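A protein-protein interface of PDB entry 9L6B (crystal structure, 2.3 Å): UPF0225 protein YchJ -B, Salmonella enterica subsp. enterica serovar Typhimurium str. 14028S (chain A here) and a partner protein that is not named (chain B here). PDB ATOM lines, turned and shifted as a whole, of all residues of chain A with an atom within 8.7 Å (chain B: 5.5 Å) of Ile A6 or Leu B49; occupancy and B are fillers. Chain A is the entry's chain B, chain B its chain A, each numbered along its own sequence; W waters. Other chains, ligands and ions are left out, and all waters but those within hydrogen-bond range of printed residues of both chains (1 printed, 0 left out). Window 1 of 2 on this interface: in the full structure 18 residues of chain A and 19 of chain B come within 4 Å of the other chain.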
ATOM      1  N   ALA A   1      14.526  23.216   3.859  1.00  0.00           N
ATOM      2  CA  ALA A   1      14.351  22.770   5.232  1.00  0.00           C
ATOM      3  C   ALA A   1      15.506  21.851   5.630  1.00  0.00           C
ATOM      4  O   ALA A   1      16.424  22.304   6.321  1.00  0.00           O
ATOM      5  CB  ALA A   1      13.012  22.084   5.406  1.00  0.00           C
ATOM      6  N   PHE A   2      15.487  20.580   5.218  1.00  0.00           N
ATOM      7  CA  PHE A   2      16.633  19.722   5.506  1.00  0.00           C
ATOM      8  C   PHE A   2      17.702  19.808   4.461  1.00  0.00           C
ATOM      9  O   PHE A   2      18.798  19.302   4.703  1.00  0.00           O
ATOM     10  CB  PHE A   2      16.386  18.208   5.471  1.00  0.00           C
ATOM     11  CG  PHE A   2      15.293  17.704   6.291  1.00  0.00           C
ATOM     12  CD1 PHE A   2      14.490  18.532   7.049  1.00  0.00           C
ATOM     13  CD2 PHE A   2      15.044  16.338   6.272  1.00  0.00           C
ATOM     14  CE1 PHE A   2      13.476  18.003   7.770  1.00  0.00           C
ATOM     15  CE2 PHE A   2      14.036  15.816   6.997  1.00  0.00           C
ATOM     16  CZ  PHE A   2      13.236  16.646   7.742  1.00  0.00           C
ATOM     17  N   ARG A   3      17.364  20.271   3.260  1.00  0.00           N
ATOM     18  CA  ARG A   3      18.187  19.925   2.115  1.00  0.00           C
ATOM     19  C   ARG A   3      19.660  20.202   2.378  1.00  0.00           C
ATOM     20  O   ARG A   3      20.513  19.349   2.106  1.00  0.00           O
ATOM     21  CB  ARG A   3      17.725  20.665   0.881  1.00  0.00           C
ATOM     22  CG  ARG A   3      18.412  20.094  -0.296  1.00  0.00           C
ATOM     23  CD  ARG A   3      18.774  21.142  -1.273  1.00  0.00           C
ATOM     24  NE  ARG A   3      19.441  20.527  -2.406  1.00  0.00           N
ATOM     25  CZ  ARG A   3      18.817  19.812  -3.326  1.00  0.00           C
ATOM     26  NH1 ARG A   3      17.511  19.600  -3.265  1.00  0.00           N
ATOM     27  NH2 ARG A   3      19.521  19.296  -4.329  1.00  0.00           N
ATOM     28  N   ASP A   4      19.973  21.356   2.982  1.00  0.00           N
ATOM     29  CA  ASP A   4      21.367  21.667   3.276  1.00  0.00           C
ATOM     30  C   ASP A   4      21.884  20.907   4.498  1.00  0.00           C
ATOM     31  O   ASP A   4      23.070  20.566   4.542  1.00  0.00           O
ATOM     32  CB  ASP A   4      21.540  23.178   3.447  1.00  0.00           C
ATOM     33  CG  ASP A   4      21.013  23.971   2.241  1.00  0.00           C
ATOM     34  OD1 ASP A   4      20.282  24.971   2.459  1.00  0.00           O
ATOM     35  OD2 ASP A   4      21.304  23.587   1.077  1.00  0.00           O
ATOM     36  N   ASP A   5      21.030  20.631   5.492  1.00  0.00           N
ATOM     37  CA  ASP A   5      21.382  19.644   6.517  1.00  0.00           C
ATOM     38  C   ASP A   5      21.856  18.341   5.882  1.00  0.00           C
ATOM     39  O   ASP A   5      22.809  17.717   6.361  1.00  0.00           O
ATOM     40  CB  ASP A   5      20.183  19.327   7.422  1.00  0.00           C
ATOM     41  CG  ASP A   5      19.872  20.422   8.419  1.00  0.00           C
ATOM     42  OD1 ASP A   5      19.834  21.612   8.023  1.00  0.00           O
ATOM     43  OD2 ASP A   5      19.622  20.070   9.598  1.00  0.00           O
ATOM     44  N   ILE A   6      21.173  17.900   4.820  1.00  0.00           N
ATOM     45  CA  ILE A   6      21.471  16.606   4.215  1.00  0.00           C
ATOM     46  C   ILE A   6      22.810  16.654   3.493  1.00  0.00           C
ATOM     47  O   ILE A   6      23.684  15.809   3.719  1.00  0.00           O
ATOM     48  CB  ILE A   6      20.341  16.178   3.258  1.00  0.00           C
ATOM     49  CG1 ILE A   6      19.030  15.939   4.009  1.00  0.00           C
ATOM     50  CG2 ILE A   6      20.744  14.940   2.483  1.00  0.00           C
ATOM     51  CD1 ILE A   6      17.845  15.730   3.074  1.00  0.00           C
ATOM     52  N   ILE A   7      22.984  17.629   2.595  1.00  0.00           N
ATOM     53  CA  ILE A   7      24.271  17.787   1.917  1.00  0.00           C
ATOM     54  C   ILE A   7      25.392  17.903   2.937  1.00  0.00           C
ATOM     55  O   ILE A   7      26.431  17.247   2.812  1.00  0.00           O
ATOM     56  CB  ILE A   7      24.236  18.993   0.961  1.00  0.00           C
ATOM     57  CG1 ILE A   7      23.079  18.835  -0.029  1.00  0.00           C
ATOM     58  CG2 ILE A   7      25.529  19.081   0.184  1.00  0.00           C
ATOM     59  CD1 ILE A   7      22.810  20.072  -0.860  1.00  0.00           C
ATOM     60  N   ALA A   8      25.168  18.676   4.005  1.00  0.00           N
ATOM     61  CA  ALA A   8      26.231  18.922   4.976  1.00  0.00           C
ATOM     62  C   ALA A   8      26.651  17.641   5.677  1.00  0.00           C
ATOM     63  O   ALA A   8      27.825  17.472   6.028  1.00  0.00           O
ATOM     64  CB  ALA A   8      25.783  19.971   5.999  1.00  0.00           C
ATOM     65  N   GLY A   9      25.706  16.717   5.886  1.00  0.00           N
ATOM     66  CA  GLY A   9      26.025  15.437   6.507  1.00  0.00           C
ATOM     67  C   GLY A   9      26.854  14.511   5.635  1.00  0.00           C
ATOM     68  O   GLY A   9      27.414  13.529   6.139  1.00  0.00           O
ATOM     69  N   PHE A  10      26.950  14.804   4.338  1.00  0.00           N
ATOM     70  CA  PHE A  10      27.769  13.984   3.449  1.00  0.00           C
ATOM     71  C   PHE A  10      29.256  14.140   3.758  1.00  0.00           C
ATOM     72  O   PHE A  10      29.994  13.149   3.811  1.00  0.00           O
ATOM     73  CB  PHE A  10      27.471  14.353   2.001  1.00  0.00           C
ATOM     74  CG  PHE A  10      26.075  13.999   1.565  1.00  0.00           C
ATOM     75  CD1 PHE A  10      25.374  12.992   2.210  1.00  0.00           C
ATOM     76  CD2 PHE A  10      25.460  14.671   0.520  1.00  0.00           C
ATOM     77  CE1 PHE A  10      24.095  12.650   1.821  1.00  0.00           C
ATOM     78  CE2 PHE A  10      24.175  14.331   0.122  1.00  0.00           C
ATOM     79  CZ  PHE A  10      23.492  13.312   0.777  1.00  0.00           C
ATOM     80  N   ALA A  11      29.709  15.371   3.998  1.00  0.00           N
ATOM     81  CA  ALA A  11      31.129  15.617   4.219  1.00  0.00           C
ATOM     82  C   ALA A  11      31.673  14.918   5.459  1.00  0.00           C
ATOM     83  O   ALA A  11      32.887  14.722   5.564  1.00  0.00           O
ATOM     84  CB  ALA A  11      31.383  17.119   4.330  1.00  0.00           C
ATOM     85  N   ASN A  12      30.817  14.521   6.392  1.00  0.00           N
ATOM     86  CA  ASN A  12      31.299  14.108   7.701  1.00  0.00           C
ATOM     87  C   ASN A  12      31.352  12.604   7.908  1.00  0.00           C
ATOM     88  O   ASN A  12      31.921  12.159   8.910  1.00  0.00           O
ATOM     89  CB  ASN A  12      30.422  14.727   8.789  1.00  0.00           C
ATOM     90  CG  ASN A  12      30.045  16.158   8.473  1.00  0.00           C
ATOM     91  OD1 ASN A  12      28.869  16.455   8.234  1.00  0.00           O
ATOM     92  ND2 ASN A  12      31.039  17.055   8.457  1.00  0.00           N
ATOM     93  N   TRP A  15      30.612   5.710   4.838  1.00  0.00           N
ATOM     94  CA  TRP A  15      29.792   4.543   5.148  1.00  0.00           C
ATOM     95  C   TRP A  15      30.510   3.265   4.745  1.00  0.00           C
ATOM     96  O   TRP A  15      31.139   3.199   3.686  1.00  0.00           O
ATOM     97  CB  TRP A  15      28.440   4.630   4.445  1.00  0.00           C
ATOM     98  CG  TRP A  15      27.630   5.785   4.909  1.00  0.00           C
ATOM     99  CD1 TRP A  15      27.450   6.975   4.266  1.00  0.00           C
ATOM    100  CD2 TRP A  15      26.904   5.876   6.142  1.00  0.00           C
ATOM    101  NE1 TRP A  15      26.643   7.791   5.022  1.00  0.00           N
ATOM    102  CE2 TRP A  15      26.302   7.139   6.178  1.00  0.00           C
ATOM    103  CE3 TRP A  15      26.703   5.000   7.216  1.00  0.00           C
ATOM    104  CZ2 TRP A  15      25.501   7.552   7.243  1.00  0.00           C
ATOM    105  CZ3 TRP A  15      25.917   5.415   8.279  1.00  0.00           C
ATOM    106  CH2 TRP A  15      25.325   6.678   8.284  1.00  0.00           C
ATOM    107  N   ARG B  37      17.764   4.044   0.391  1.00  0.00           N
ATOM    108  CA  ARG B  37      18.178   5.281   1.054  1.00  0.00           C
ATOM    109  C   ARG B  37      19.601   5.171   1.584  1.00  0.00           C
ATOM    110  O   ARG B  37      20.333   6.162   1.595  1.00  0.00           O
ATOM    111  CB  ARG B  37      17.226   5.635   2.207  1.00  0.00           C
ATOM    112  CG  ARG B  37      15.783   6.002   1.788  1.00  0.00           C
ATOM    113  CD  ARG B  37      14.877   6.215   3.010  1.00  0.00           C
ATOM    114  NE  ARG B  37      15.356   7.236   3.940  1.00  0.00           N
ATOM    115  CZ  ARG B  37      15.130   8.532   3.796  1.00  0.00           C
ATOM    116  NH1 ARG B  37      14.474   9.009   2.752  1.00  0.00           N
ATOM    117  NH2 ARG B  37      15.585   9.378   4.719  1.00  0.00           N
ATOM    118  N   ALA B  40      21.640   6.056  -1.349  1.00  0.00           N
ATOM    119  CA  ALA B  40      21.645   7.501  -1.558  1.00  0.00           C
ATOM    120  C   ALA B  40      22.538   8.226  -0.557  1.00  0.00           C
ATOM    121  O   ALA B  40      23.102   9.273  -0.884  1.00  0.00           O
ATOM    122  CB  ALA B  40      20.221   8.057  -1.495  1.00  0.00           C
ATOM    123  N   PHE B  41      22.691   7.704   0.659  1.00  0.00           N
ATOM    124  CA  PHE B  41      23.660   8.304   1.574  1.00  0.00           C
ATOM    125  C   PHE B  41      25.087   8.055   1.095  1.00  0.00           C
ATOM    126  O   PHE B  41      25.927   8.966   1.097  1.00  0.00           O
ATOM    127  CB  PHE B  41      23.475   7.753   2.985  1.00  0.00           C
ATOM    128  CG  PHE B  41      22.457   8.490   3.788  1.00  0.00           C
ATOM    129  CD1 PHE B  41      22.697   9.790   4.207  1.00  0.00           C
ATOM    130  CD2 PHE B  41      21.268   7.883   4.141  1.00  0.00           C
ATOM    131  CE1 PHE B  41      21.756  10.474   4.950  1.00  0.00           C
ATOM    132  CE2 PHE B  41      20.317   8.563   4.887  1.00  0.00           C
ATOM    133  CZ  PHE B  41      20.559   9.856   5.294  1.00  0.00           C
ATOM    134  N   ASP B  45      23.314  11.395  -2.816  1.00  0.00           N
ATOM    135  CA  ASP B  45      22.168  11.825  -3.624  1.00  0.00           C
ATOM    136  C   ASP B  45      21.102  12.424  -2.701  1.00  0.00           C
ATOM    137  O   ASP B  45      20.166  11.737  -2.278  1.00  0.00           O
ATOM    138  CB  ASP B  45      21.619  10.642  -4.421  1.00  0.00           C
ATOM    139  CG  ASP B  45      20.479  11.030  -5.361  1.00  0.00           C
ATOM    140  OD1 ASP B  45      19.982  12.171  -5.260  1.00  0.00           O
ATOM    141  OD2 ASP B  45      20.090  10.194  -6.219  1.00  0.00           O
ATOM    142  N   ALA B  46      21.221  13.732  -2.424  1.00  0.00           N
ATOM    143  CA  ALA B  46      20.284  14.390  -1.516  1.00  0.00           C
ATOM    144  C   ALA B  46      18.867  14.412  -2.069  1.00  0.00           C
ATOM    145  O   ALA B  46      17.909  14.345  -1.298  1.00  0.00           O
ATOM    146  CB  ALA B  46      20.745  15.814  -1.215  1.00  0.00           C
ATOM    147  N   ASP B  47      18.702  14.492  -3.390  1.00  0.00           N
ATOM    148  CA  ASP B  47      17.355  14.597  -3.946  1.00  0.00           C
ATOM    149  C   ASP B  47      16.564  13.307  -3.758  1.00  0.00           C
ATOM    150  O   ASP B  47      15.353  13.355  -3.520  1.00  0.00           O
ATOM    151  CB  ASP B  47      17.424  14.985  -5.421  1.00  0.00           C
ATOM    152  CG  ASP B  47      17.995  16.387  -5.627  1.00  0.00           C
ATOM    153  OD1 ASP B  47      17.694  17.295  -4.811  1.00  0.00           O
ATOM    154  OD2 ASP B  47      18.754  16.584  -6.594  1.00  0.00           O
ATOM    155  N   TYR B  48      17.214  12.143  -3.854  1.00  0.00           N
ATOM    156  CA  TYR B  48      16.467  10.912  -3.619  1.00  0.00           C
ATOM    157  C   TYR B  48      16.075  10.783  -2.154  1.00  0.00           C
ATOM    158  O   TYR B  48      15.001  10.262  -1.841  1.00  0.00           O
ATOM    159  CB  TYR B  48      17.244   9.658  -4.053  1.00  0.00           C
ATOM    160  CG  TYR B  48      16.427   8.426  -3.710  1.00  0.00           C
ATOM    161  CD1 TYR B  48      15.243   8.167  -4.378  1.00  0.00           C
ATOM    162  CD2 TYR B  48      16.781   7.586  -2.654  1.00  0.00           C
ATOM    163  CE1 TYR B  48      14.449   7.075  -4.043  1.00  0.00           C
ATOM    164  CE2 TYR B  48      15.986   6.482  -2.308  1.00  0.00           C
ATOM    165  CZ  TYR B  48      14.821   6.242  -3.013  1.00  0.00           C
ATOM    166  OH  TYR B  48      14.015   5.170  -2.701  1.00  0.00           O
ATOM    167  N   LEU B  49      16.942  11.221  -1.238  1.00  0.00           N
ATOM    168  CA  LEU B  49      16.584  11.184   0.176  1.00  0.00           C
ATOM    169  C   LEU B  49      15.386  12.070   0.459  1.00  0.00           C
ATOM    170  O   LEU B  49      14.470  11.683   1.196  1.00  0.00           O
ATOM    171  CB  LEU B  49      17.766  11.621   1.023  1.00  0.00           C
ATOM    172  CG  LEU B  49      18.928  10.650   0.904  1.00  0.00           C
ATOM    173  CD1 LEU B  49      20.159  11.222   1.589  1.00  0.00           C
ATOM    174  CD2 LEU B  49      18.525   9.338   1.525  1.00  0.00           C
ATOM    175  N   ILE B  50      15.382  13.267  -0.113  1.00  0.00           N
ATOM    176  CA  ILE B  50      14.235  14.148   0.050  1.00  0.00           C
ATOM    177  C   ILE B  50      12.981  13.468  -0.474  1.00  0.00           C
ATOM    178  O   ILE B  50      11.962  13.399   0.218  1.00  0.00           O
ATOM    179  CB  ILE B  50      14.495  15.488  -0.654  1.00  0.00           C
ATOM    180  CG1 ILE B  50      15.536  16.272   0.130  1.00  0.00           C
ATOM    181  CG2 ILE B  50      13.199  16.260  -0.820  1.00  0.00           C
ATOM    182  CD1 ILE B  50      16.257  17.307  -0.693  1.00  0.00           C
ATOM    183  N   LYS B  51      13.061  12.895  -1.681  1.00  0.00           N
ATOM    184  CA  LYS B  51      11.895  12.302  -2.326  1.00  0.00           C
ATOM    185  C   LYS B  51      11.366  11.061  -1.600  1.00  0.00           C
ATOM    186  O   LYS B  51      10.179  10.730  -1.748  1.00  0.00           O
ATOM    187  CB  LYS B  51      12.226  11.935  -3.782  1.00  0.00           C
ATOM    188  CG  LYS B  51      11.013  11.641  -4.665  1.00  0.00           C
ATOM    189  CD  LYS B  51      11.168  10.341  -5.456  1.00  0.00           C
ATOM    190  CE  LYS B  51      11.059   9.089  -4.553  1.00  0.00           C
ATOM    191  NZ  LYS B  51      10.916   7.780  -5.343  1.00  0.00           N
ATOM    192  N   SER B  52      12.205  10.351  -0.844  1.00  0.00           N
ATOM    193  CA  SER B  52      11.746   9.173  -0.122  1.00  0.00           C
ATOM    194  C   SER B  52      11.443   9.455   1.344  1.00  0.00           C
ATOM    195  O   SER B  52      11.065   8.530   2.069  1.00  0.00           O
ATOM    196  CB  SER B  52      12.767   8.027  -0.242  1.00  0.00           C
ATOM    197  OG  SER B  52      14.082   8.457   0.049  1.00  0.00           O
ATOM    198  N   TRP B  53      11.581  10.706   1.785  1.00  0.00           N
ATOM    199  CA  TRP B  53      11.135  11.117   3.112  1.00  0.00           C
ATOM    200  C   TRP B  53       9.631  11.406   3.094  1.00  0.00           C
ATOM    201  O   TRP B  53       9.126  12.076   2.185  1.00  0.00           O
ATOM    202  CB  TRP B  53      11.903  12.371   3.569  1.00  0.00           C
ATOM    203  CG  TRP B  53      12.436  12.257   4.944  1.00  0.00           C
ATOM    204  CD1 TRP B  53      11.718  12.022   6.075  1.00  0.00           C
ATOM    205  CD2 TRP B  53      13.808  12.363   5.351  1.00  0.00           C
ATOM    206  NE1 TRP B  53      12.557  11.966   7.164  1.00  0.00           N
ATOM    207  CE2 TRP B  53      13.844  12.177   6.747  1.00  0.00           C
ATOM    208  CE3 TRP B  53      15.009  12.610   4.673  1.00  0.00           C
ATOM    209  CZ2 TRP B  53      15.029  12.215   7.478  1.00  0.00           C
ATOM    210  CZ3 TRP B  53      16.180  12.645   5.396  1.00  0.00           C
ATOM    211  CH2 TRP B  53      16.186  12.446   6.784  1.00  0.00           C
ATOM    212  N   ALA B  59      11.027  17.575   3.925  1.00  0.00           N
ATOM    213  CA  ALA B  59      12.468  17.357   3.766  1.00  0.00           C
ATOM    214  C   ALA B  59      13.130  18.374   2.829  1.00  0.00           C
ATOM    215  O   ALA B  59      14.321  18.673   2.986  1.00  0.00           O
ATOM    216  CB  ALA B  59      12.714  15.930   3.259  1.00  0.00           C
HETATM  217  O   HOH W   1      26.225  10.336   3.848  1.00  0.00           O
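The guanidinium group (NH1) of Arg B37 is in hydrogen-bond range of the backbone carbonyl oxygen (O) of Leu B49 (3.1 Å). The side-chain carboxylate (OD1) of Asp B45 lies close to the backbone NH (N) of Asp B47. The backbone carbonyl oxygen (O) of Leu B49 sits at hydrogen-bond distance from the side-chain hydroxyl (OG) of Ser B52.
The guanidinium group (NH2) of Arg A3 lies within salt-bridge range of the side-chain carboxylate (OD1) of Asp B47, 2.8 Å away. The backbone carbonyl oxygen (O) of Ala B59 is in hydrogen-bond range of the backbone NH (N) of Phe A2 (3.2 Å). The backbone carbonyl oxygen (O) of Ala B59 is in hydrogen-bond range of the backbone NH (N) of Arg A3.
Water W1 bridges the indole nitrogen of Trp A15 (2.8 Å) and the backbone carbonyl oxygen of Phe B41 (3.1 Å).
Of the 13 printed residues of chain A, 6 touch a printed residue of chain B. Printed residues of chain A that touch a printed residue of chain B: Phe A2, Arg A3, Ile A6, Ile A7, Phe A10 and Trp A15. Hydrophobic or aromatic side chains of chain A within 4 Å of the printed part of chain B: Phe A2, Ile A6, Ile A7, Phe A10 and Trp A15. Among the printed residues, Asp or Glu carboxylates within 4 Å of a Lys or Arg side-chain nitrogen of the other chain: Arg A3 with Asp B47.
Printed residues of chain B within 4 Å of Ile A6: Ala B46 (3.8 Å), Leu B49 (3.9 Å) and Ile B50 (3.8 Å). Of the printed residues of chain A, Leu B49 touches Ile A6. Of the printed residues of chain B, Phe A2 touches Trp B53 and Ala B59. Of the printed residues of chain B, Ile A7 touches Ala B46. Printed residues of chain B within 4 Å of Phe A10: Phe B41 (3.98 Å) and Ala B46 (3.9 Å). Asp A5 touches none of the printed residues of chain B. Tyr B48 touches none of the printed residues of chain A.
Among the printed residues, merely in contact across the chains: Arg A3 with Ile B50 (3.5 Å), Phe A2 with Trp B53 (3.7 Å), Trp A15 with Phe B41 (3.8 Å), Ile A6 with Ile B50 (3.8 Å), Ile A6 with Ala B46 (3.8 Å), Ile A6 with Leu B49 (3.9 Å), Phe A10 with Ala B46 (3.9 Å), Phe A10 with Phe B41 (3.98 Å) and Ile A7 with Ala B46 (3.998 Å).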
